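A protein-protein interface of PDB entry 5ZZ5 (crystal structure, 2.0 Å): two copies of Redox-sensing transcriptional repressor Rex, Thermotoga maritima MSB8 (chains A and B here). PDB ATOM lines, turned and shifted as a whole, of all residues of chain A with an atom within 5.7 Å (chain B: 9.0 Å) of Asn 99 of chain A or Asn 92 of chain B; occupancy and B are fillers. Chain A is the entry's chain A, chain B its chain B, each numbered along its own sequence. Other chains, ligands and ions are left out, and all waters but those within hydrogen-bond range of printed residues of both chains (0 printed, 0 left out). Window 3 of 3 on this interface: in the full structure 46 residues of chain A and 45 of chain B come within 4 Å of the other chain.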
ATOM      1  N   GLY A  94      26.469 -27.948 -25.274  1.00  0.00           N
ATOM      2  CA  GLY A  94      25.446 -27.939 -24.235  1.00  0.00           C
ATOM      3  C   GLY A  94      25.510 -26.726 -23.327  1.00  0.00           C
ATOM      4  O   GLY A  94      24.474 -26.129 -22.996  1.00  0.00           O
ATOM      5  N   ARG A  95      26.725 -26.367 -22.900  1.00  0.00           N
ATOM      6  CA  ARG A  95      26.922 -25.146 -22.130  1.00  0.00           C
ATOM      7  C   ARG A  95      26.469 -23.954 -22.957  1.00  0.00           C
ATOM      8  O   ARG A  95      25.776 -23.065 -22.461  1.00  0.00           O
ATOM      9  CB  ARG A  95      28.390 -24.973 -21.716  1.00  0.00           C
ATOM     10  CG  ARG A  95      28.847 -25.867 -20.569  1.00  0.00           C
ATOM     11  CD  ARG A  95      30.290 -25.565 -20.145  1.00  0.00           C
ATOM     12  NE  ARG A  95      31.294 -26.222 -20.987  1.00  0.00           N
ATOM     13  CZ  ARG A  95      32.043 -25.597 -21.896  1.00  0.00           C
ATOM     14  NH1 ARG A  95      31.913 -24.293 -22.098  1.00  0.00           N
ATOM     15  NH2 ARG A  95      32.933 -26.277 -22.606  1.00  0.00           N
ATOM     16  N   ALA A  96      26.865 -23.942 -24.230  1.00  0.00           N
ATOM     17  CA  ALA A  96      26.503 -22.831 -25.112  1.00  0.00           C
ATOM     18  C   ALA A  96      24.979 -22.675 -25.244  1.00  0.00           C
ATOM     19  O   ALA A  96      24.465 -21.557 -25.210  1.00  0.00           O
ATOM     20  CB  ALA A  96      27.145 -23.004 -26.479  1.00  0.00           C
ATOM     21  N   VAL A  97      24.254 -23.783 -25.392  1.00  0.00           N
ATOM     22  CA  VAL A  97      22.791 -23.681 -25.466  1.00  0.00           C
ATOM     23  C   VAL A  97      22.210 -23.203 -24.131  1.00  0.00           C
ATOM     24  O   VAL A  97      21.323 -22.337 -24.103  1.00  0.00           O
ATOM     25  CB  VAL A  97      22.133 -25.027 -25.869  1.00  0.00           C
ATOM     26  CG1 VAL A  97      20.599 -24.909 -25.848  1.00  0.00           C
ATOM     27  CG2 VAL A  97      22.592 -25.427 -27.262  1.00  0.00           C
ATOM     28  N   ALA A  98      22.757 -23.721 -23.030  1.00  0.00           N
ATOM     29  CA  ALA A  98      22.280 -23.356 -21.700  1.00  0.00           C
ATOM     30  C   ALA A  98      22.421 -21.862 -21.453  1.00  0.00           C
ATOM     31  O   ALA A  98      21.624 -21.265 -20.734  1.00  0.00           O
ATOM     32  CB  ALA A  98      23.043 -24.143 -20.623  1.00  0.00           C
ATOM     33  N   ASN A  99      23.420 -21.248 -22.078  1.00  0.00           N
ATOM     34  CA  ASN A  99      23.642 -19.830 -21.881  1.00  0.00           C
ATOM     35  C   ASN A  99      23.045 -18.961 -22.975  1.00  0.00           C
ATOM     36  O   ASN A  99      23.265 -17.747 -22.996  1.00  0.00           O
ATOM     37  CB  ASN A  99      25.140 -19.562 -21.747  1.00  0.00           C
ATOM     38  CG  ASN A  99      25.688 -20.041 -20.419  1.00  0.00           C
ATOM     39  OD1 ASN A  99      25.563 -19.355 -19.401  1.00  0.00           O
ATOM     40  ND2 ASN A  99      26.268 -21.238 -20.415  1.00  0.00           N
ATOM     41  N   TYR A 100      22.279 -19.574 -23.874  1.00  0.00           N
ATOM     42  CA  TYR A 100      21.647 -18.817 -24.943  1.00  0.00           C
ATOM     43  C   TYR A 100      20.332 -18.220 -24.463  1.00  0.00           C
ATOM     44  O   TYR A 100      19.291 -18.840 -24.583  1.00  0.00           O
ATOM     45  CB  TYR A 100      21.399 -19.693 -26.163  1.00  0.00           C
ATOM     46  CG  TYR A 100      20.988 -18.880 -27.352  1.00  0.00           C
ATOM     47  CD1 TYR A 100      21.783 -17.836 -27.805  1.00  0.00           C
ATOM     48  CD2 TYR A 100      19.801 -19.130 -28.010  1.00  0.00           C
ATOM     49  CE1 TYR A 100      21.411 -17.079 -28.894  1.00  0.00           C
ATOM     50  CE2 TYR A 100      19.423 -18.375 -29.097  1.00  0.00           C
ATOM     51  CZ  TYR A 100      20.233 -17.360 -29.539  1.00  0.00           C
ATOM     52  OH  TYR A 100      19.843 -16.612 -30.626  1.00  0.00           O
ATOM     53  N   THR A 101      20.376 -17.009 -23.925  1.00  0.00           N
ATOM     54  CA  THR A 101      19.230 -16.472 -23.193  1.00  0.00           C
ATOM     55  C   THR A 101      18.035 -16.028 -24.045  1.00  0.00           C
ATOM     56  O   THR A 101      16.915 -16.013 -23.544  1.00  0.00           O
ATOM     57  CB  THR A 101      19.657 -15.283 -22.298  1.00  0.00           C
ATOM     58  OG1 THR A 101      20.514 -14.400 -23.034  1.00  0.00           O
ATOM     59  CG2 THR A 101      20.409 -15.790 -21.083  1.00  0.00           C
ATOM     60  N   ALA A 125      26.331 -24.979 -15.177  1.00  0.00           N
ATOM     61  CA  ALA A 125      26.477 -24.776 -16.619  1.00  0.00           C
ATOM     62  C   ALA A 125      26.127 -23.345 -17.028  1.00  0.00           C
ATOM     63  O   ALA A 125      26.691 -22.801 -17.979  1.00  0.00           O
ATOM     64  CB  ALA A 125      25.601 -25.770 -17.372  1.00  0.00           C
ATOM     65  N   ALA A 126      25.193 -22.749 -16.298  1.00  0.00           N
ATOM     66  CA  ALA A 126      24.709 -21.403 -16.576  1.00  0.00           C
ATOM     67  C   ALA A 126      24.183 -20.798 -15.274  1.00  0.00           C
ATOM     68  O   ALA A 126      24.042 -21.511 -14.285  1.00  0.00           O
ATOM     69  CB  ALA A 126      23.621 -21.434 -17.637  1.00  0.00           C
ATOM     70  N   PRO A 127      23.937 -19.477 -15.251  1.00  0.00           N
ATOM     71  CA  PRO A 127      23.370 -18.874 -14.038  1.00  0.00           C
ATOM     72  C   PRO A 127      22.046 -19.500 -13.618  1.00  0.00           C
ATOM     73  O   PRO A 127      21.088 -19.466 -14.384  1.00  0.00           O
ATOM     74  CB  PRO A 127      23.176 -17.413 -14.441  1.00  0.00           C
ATOM     75  CG  PRO A 127      24.285 -17.169 -15.405  1.00  0.00           C
ATOM     76  CD  PRO A 127      24.376 -18.444 -16.208  1.00  0.00           C
ATOM     77  N   VAL B  87      35.951 -16.521 -37.284  1.00  0.00           N
ATOM     78  CA  VAL B  87      34.775 -16.265 -36.466  1.00  0.00           C
ATOM     79  C   VAL B  87      34.832 -14.822 -36.010  1.00  0.00           C
ATOM     80  O   VAL B  87      35.903 -14.363 -35.572  1.00  0.00           O
ATOM     81  CB  VAL B  87      34.748 -17.187 -35.251  1.00  0.00           C
ATOM     82  CG1 VAL B  87      33.571 -16.843 -34.340  1.00  0.00           C
ATOM     83  CG2 VAL B  87      34.728 -18.673 -35.706  1.00  0.00           C
ATOM     84  N   GLY B  89      33.136 -12.358 -33.314  1.00  0.00           N
ATOM     85  CA  GLY B  89      32.353 -12.436 -32.096  1.00  0.00           C
ATOM     86  C   GLY B  89      32.937 -13.529 -31.244  1.00  0.00           C
ATOM     87  O   GLY B  89      32.858 -14.691 -31.604  1.00  0.00           O
ATOM     88  N   ALA B  90      33.548 -13.153 -30.119  1.00  0.00           N
ATOM     89  CA  ALA B  90      34.162 -14.130 -29.241  1.00  0.00           C
ATOM     90  C   ALA B  90      33.353 -14.296 -27.961  1.00  0.00           C
ATOM     91  O   ALA B  90      33.909 -14.438 -26.877  1.00  0.00           O
ATOM     92  CB  ALA B  90      35.585 -13.743 -28.920  1.00  0.00           C
ATOM     93  N   GLY B  91      32.038 -14.227 -28.093  1.00  0.00           N
ATOM     94  CA  GLY B  91      31.143 -14.468 -26.978  1.00  0.00           C
ATOM     95  C   GLY B  91      30.774 -15.940 -26.875  1.00  0.00           C
ATOM     96  O   GLY B  91      31.522 -16.813 -27.316  1.00  0.00           O
ATOM     97  N   ASN B  92      29.599 -16.198 -26.318  1.00  0.00           N
ATOM     98  CA  ASN B  92      29.101 -17.552 -26.047  1.00  0.00           C
ATOM     99  C   ASN B  92      29.151 -18.452 -27.285  1.00  0.00           C
ATOM    100  O   ASN B  92      29.778 -19.514 -27.290  1.00  0.00           O
ATOM    101  CB  ASN B  92      27.665 -17.458 -25.518  1.00  0.00           C
ATOM    102  CG  ASN B  92      27.067 -18.814 -25.164  1.00  0.00           C
ATOM    103  OD1 ASN B  92      27.750 -19.695 -24.645  1.00  0.00           O
ATOM    104  ND2 ASN B  92      25.774 -18.978 -25.438  1.00  0.00           N
ATOM    105  N   ILE B  93      28.512 -17.988 -28.346  1.00  0.00           N
ATOM    106  CA  ILE B  93      28.461 -18.730 -29.591  1.00  0.00           C
ATOM    107  C   ILE B  93      29.806 -18.809 -30.316  1.00  0.00           C
ATOM    108  O   ILE B  93      30.221 -19.894 -30.751  1.00  0.00           O
ATOM    109  CB  ILE B  93      27.425 -18.094 -30.514  1.00  0.00           C
ATOM    110  CG1 ILE B  93      26.032 -18.262 -29.884  1.00  0.00           C
ATOM    111  CG2 ILE B  93      27.540 -18.684 -31.894  1.00  0.00           C
ATOM    112  CD1 ILE B  93      24.934 -17.403 -30.511  1.00  0.00           C
ATOM    113  N   GLY B  94      30.497 -17.670 -30.426  1.00  0.00           N
ATOM    114  CA  GLY B  94      31.765 -17.631 -31.133  1.00  0.00           C
ATOM    115  C   GLY B  94      32.763 -18.593 -30.529  1.00  0.00           C
ATOM    116  O   GLY B  94      33.407 -19.354 -31.251  1.00  0.00           O
ATOM    117  N   ARG B  95      32.864 -18.586 -29.196  1.00  0.00           N
ATOM    118  CA  ARG B  95      33.805 -19.454 -28.502  1.00  0.00           C
ATOM    119  C   ARG B  95      33.413 -20.912 -28.671  1.00  0.00           C
ATOM    120  O   ARG B  95      34.265 -21.772 -28.903  1.00  0.00           O
ATOM    121  CB  ARG B  95      33.884 -19.089 -27.018  1.00  0.00           C
ATOM    122  CG  ARG B  95      34.478 -17.704 -26.756  1.00  0.00           C
ATOM    123  CD  ARG B  95      34.460 -17.363 -25.270  1.00  0.00           C
ATOM    124  NE  ARG B  95      35.417 -18.193 -24.557  1.00  0.00           N
ATOM    125  CZ  ARG B  95      36.702 -17.881 -24.411  1.00  0.00           C
ATOM    126  NH1 ARG B  95      37.170 -16.754 -24.932  1.00  0.00           N
ATOM    127  NH2 ARG B  95      37.516 -18.693 -23.747  1.00  0.00           N
ATOM    128  N   ALA B  96      32.122 -21.186 -28.563  1.00  0.00           N
ATOM    129  CA  ALA B  96      31.624 -22.543 -28.754  1.00  0.00           C
ATOM    130  C   ALA B  96      32.010 -23.055 -30.143  1.00  0.00           C
ATOM    131  O   ALA B  96      32.474 -24.185 -30.274  1.00  0.00           O
ATOM    132  CB  ALA B  96      30.124 -22.589 -28.569  1.00  0.00           C
ATOM    133  N   VAL B  97      31.847 -22.211 -31.167  1.00  0.00           N
ATOM    134  CA  VAL B  97      32.235 -22.602 -32.523  1.00  0.00           C
ATOM    135  C   VAL B  97      33.743 -22.783 -32.617  1.00  0.00           C
ATOM    136  O   VAL B  97      34.204 -23.730 -33.259  1.00  0.00           O
ATOM    137  CB  VAL B  97      31.729 -21.589 -33.607  1.00  0.00           C
ATOM    138  CG1 VAL B  97      32.293 -21.929 -35.010  1.00  0.00           C
ATOM    139  CG2 VAL B  97      30.190 -21.575 -33.653  1.00  0.00           C
ATOM    140  N   ALA B  98      34.512 -21.895 -31.972  1.00  0.00           N
ATOM    141  CA  ALA B  98      35.965 -22.021 -31.973  1.00  0.00           C
ATOM    142  C   ALA B  98      36.419 -23.312 -31.308  1.00  0.00           C
ATOM    143  O   ALA B  98      37.469 -23.848 -31.665  1.00  0.00           O
ATOM    144  CB  ALA B  98      36.640 -20.791 -31.289  1.00  0.00           C
ATOM    145  N   ASN B  99      35.653 -23.818 -30.341  1.00  0.00           N
ATOM    146  CA  ASN B  99      36.005 -25.081 -29.677  1.00  0.00           C
ATOM    147  C   ASN B  99      35.284 -26.319 -30.230  1.00  0.00           C
ATOM    148  O   ASN B  99      35.341 -27.411 -29.637  1.00  0.00           O
ATOM    149  CB  ASN B  99      35.721 -24.985 -28.183  1.00  0.00           C
ATOM    150  CG  ASN B  99      36.721 -24.124 -27.467  1.00  0.00           C
ATOM    151  OD1 ASN B  99      37.817 -24.572 -27.159  1.00  0.00           O
ATOM    152  ND2 ASN B  99      36.357 -22.879 -27.207  1.00  0.00           N
ATOM    153  N   ILE B 113      39.853 -15.589 -34.878  1.00  0.00           N
ATOM    154  CA  ILE B 113      38.606 -15.208 -34.248  1.00  0.00           C
ATOM    155  C   ILE B 113      38.754 -13.776 -33.759  1.00  0.00           C
ATOM    156  O   ILE B 113      39.806 -13.380 -33.252  1.00  0.00           O
ATOM    157  CB  ILE B 113      38.226 -16.170 -33.111  1.00  0.00           C
ATOM    158  CG1 ILE B 113      36.966 -15.686 -32.377  1.00  0.00           C
ATOM    159  CG2 ILE B 113      39.394 -16.364 -32.158  1.00  0.00           C
ATOM    160  CD1 ILE B 113      36.298 -16.746 -31.468  1.00  0.00           C
ATOM    161  N   ASP B 115      37.115  -9.925 -32.215  1.00  0.00           N
ATOM    162  CA  ASP B 115      36.168  -9.216 -31.381  1.00  0.00           C
ATOM    163  C   ASP B 115      36.569  -7.748 -31.225  1.00  0.00           C
ATOM    164  O   ASP B 115      37.719  -7.371 -31.486  1.00  0.00           O
ATOM    165  CB  ASP B 115      36.050  -9.914 -30.036  1.00  0.00           C
ATOM    166  CG  ASP B 115      34.734  -9.651 -29.360  1.00  0.00           C
ATOM    167  OD1 ASP B 115      34.623  -8.577 -28.731  1.00  0.00           O
ATOM    168  OD2 ASP B 115      33.820 -10.505 -29.454  1.00  0.00           O
ATOM    169  N   LYS B 120      38.346  -8.892 -24.284  1.00  0.00           N
ATOM    170  CA  LYS B 120      38.341 -10.191 -24.941  1.00  0.00           C
ATOM    171  C   LYS B 120      39.584 -10.404 -25.813  1.00  0.00           C
ATOM    172  O   LYS B 120      40.151 -11.501 -25.858  1.00  0.00           O
ATOM    173  CB  LYS B 120      37.059 -10.372 -25.795  1.00  0.00           C
ATOM    174  CG  LYS B 120      35.830 -10.790 -24.970  1.00  0.00           C
ATOM    175  CD  LYS B 120      34.504 -10.740 -25.776  1.00  0.00           C
ATOM    176  CE  LYS B 120      33.295 -10.962 -24.859  1.00  0.00           C
ATOM    177  NZ  LYS B 120      32.437  -9.743 -24.690  1.00  0.00           N
ATOM    178  N   ALA B 125      40.634 -18.002 -27.109  1.00  0.00           N
ATOM    179  CA  ALA B 125      39.252 -18.463 -27.315  1.00  0.00           C
ATOM    180  C   ALA B 125      39.206 -19.994 -27.294  1.00  0.00           C
ATOM    181  O   ALA B 125      38.235 -20.607 -26.848  1.00  0.00           O
ATOM    182  CB  ALA B 125      38.690 -17.922 -28.631  1.00  0.00           C
ATOM    183  N   ALA B 152      29.087 -14.277 -35.374  1.00  0.00           N
ATOM    184  CA  ALA B 152      28.557 -14.622 -34.054  1.00  0.00           C
ATOM    185  C   ALA B 152      28.525 -13.388 -33.185  1.00  0.00           C
ATOM    186  O   ALA B 152      28.978 -13.401 -32.024  1.00  0.00           O
ATOM    187  CB  ALA B 152      29.389 -15.755 -33.396  1.00  0.00           C
ATOM    188  N   VAL B 153      28.016 -12.307 -33.766  1.00  0.00           N
ATOM    189  CA  VAL B 153      27.854 -11.045 -33.041  1.00  0.00           C
ATOM    190  C   VAL B 153      26.362 -10.810 -32.896  1.00  0.00           C
ATOM    191  O   VAL B 153      25.565 -11.524 -33.526  1.00  0.00           O
ATOM    192  CB  VAL B 153      28.537  -9.843 -33.766  1.00  0.00           C
ATOM    193  CG1 VAL B 153      30.047 -10.050 -33.872  1.00  0.00           C
ATOM    194  CG2 VAL B 153      27.909  -9.590 -35.126  1.00  0.00           C
ATOM    195  N   PRO B 154      25.967  -9.872 -32.016  1.00  0.00           N
ATOM    196  CA  PRO B 154      24.541  -9.536 -31.905  1.00  0.00           C
ATOM    197  C   PRO B 154      23.965  -8.972 -33.203  1.00  0.00           C
ATOM    198  O   PRO B 154      24.711  -8.441 -34.034  1.00  0.00           O
ATOM    199  CB  PRO B 154      24.517  -8.484 -30.790  1.00  0.00           C
ATOM    200  CG  PRO B 154      25.710  -8.816 -29.951  1.00  0.00           C
ATOM    201  CD  PRO B 154      26.760  -9.258 -30.931  1.00  0.00           C
ATOM    202  N   PHE B 176      25.025 -16.870 -37.374  1.00  0.00           N
ATOM    203  CA  PHE B 176      24.320 -17.170 -36.122  1.00  0.00           C
ATOM    204  C   PHE B 176      23.534 -15.985 -35.568  1.00  0.00           C
ATOM    205  O   PHE B 176      22.839 -16.127 -34.565  1.00  0.00           O
ATOM    206  CB  PHE B 176      25.288 -17.605 -35.027  1.00  0.00           C
ATOM    207  CG  PHE B 176      25.846 -18.960 -35.212  1.00  0.00           C
ATOM    208  CD1 PHE B 176      25.194 -20.072 -34.710  1.00  0.00           C
ATOM    209  CD2 PHE B 176      27.039 -19.132 -35.879  1.00  0.00           C
ATOM    210  CE1 PHE B 176      25.732 -21.326 -34.862  1.00  0.00           C
ATOM    211  CE2 PHE B 176      27.585 -20.400 -36.030  1.00  0.00           C
ATOM    212  CZ  PHE B 176      26.924 -21.492 -35.526  1.00  0.00           C
ATOM    213  N   ILE B 192      18.907 -21.315 -33.294  1.00  0.00           N
ATOM    214  CA  ILE B 192      18.322 -22.361 -32.472  1.00  0.00           C
ATOM    215  C   ILE B 192      16.841 -22.057 -32.244  1.00  0.00           C
ATOM    216  O   ILE B 192      16.030 -22.982 -32.215  1.00  0.00           O
ATOM    217  CB  ILE B 192      19.043 -22.572 -31.127  1.00  0.00           C
ATOM    218  CG1 ILE B 192      18.500 -23.833 -30.449  1.00  0.00           C
ATOM    219  CG2 ILE B 192      18.840 -21.413 -30.215  1.00  0.00           C
ATOM    220  CD1 ILE B 192      19.107 -24.123 -29.133  1.00  0.00           C
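ND2 of Asn 92 of chain B sits at hydrogen-bond distance from O of Ala 96 of chain A, 2.9 Å away.
The side-chain amide nitrogen (ND2) of Asn 99 of chain A sits at hydrogen-bond distance from the backbone carbonyl oxygen (O) of Arg 95 of chain A, at 2.8 Å.
The side-chain amide nitrogen (ND2) of Asn 99 of chain A is in hydrogen-bond range of the backbone carbonyl oxygen (O) of Ala 125 of chain A, 2.9 Å away.
Among the printed residues, pairs that only touch across the chains: Ala 96 of chain A with Ala 96 of chain B (3.7 Å), Val 97 of chain A with Ile 192 of chain B (3.7 Å), Asn 99 of chain A with Asn 92 of chain B (3.7 Å), Tyr 100 of chain A with Asn 92 of chain B (3.9 Å), Tyr 100 of chain A with Ile 93 of chain B (3.9 Å) and Tyr 100 of chain A with Ile 192 of chain B (3.3 Å).
Asn 99 of chain A touches just one residue of chain B: Asn 92 (3.7 Å).
Asn 92 of chain B touches three residues of chain A.
Of the printed residues of chain A, Ile 192 of chain B touches Val 97 (3.7 Å) and Tyr 100 (3.3 Å).
Printed residues of chain B within 4 Å of Tyr 100 of chain A: Asn 92 (3.9 Å), Ile 93 (3.9 Å) and Ile 192 (3.3 Å).
Of the printed residues of chain B, Val 97 of chain A touches Ile 192.
Of the printed residues of chain A, Ala 96 of chain B touches Ala 96 (3.7 Å).
Asn 99 of chain B touches none of the printed residues of chain A.
The nearest printed residue of chain A that does not touch Ile 192 of chain B is Ala 96 of chain A (7.1 Å).
Hydrophobic or aromatic side chains of chain B that line the printed part of chain A: Ile 93, Ala 96 and Ile 192.
Of the 11 printed residues of chain A, 4 touch a printed residue of chain B.
Hydrophobic or aromatic side chains of chain A within 4 Å of the printed part of chain B: Ala 96, Val 97 and Tyr 100.
Ala 96 of chain A touches its own counterpart, Ala 96 of chain B.
Positions printed for both chains: 94, 95, 96, 97, 98, 99 and 125.
Of the 7 pairs that touch across the chains among the printed residues, 1 has its exchanged pair printed and touching as well.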
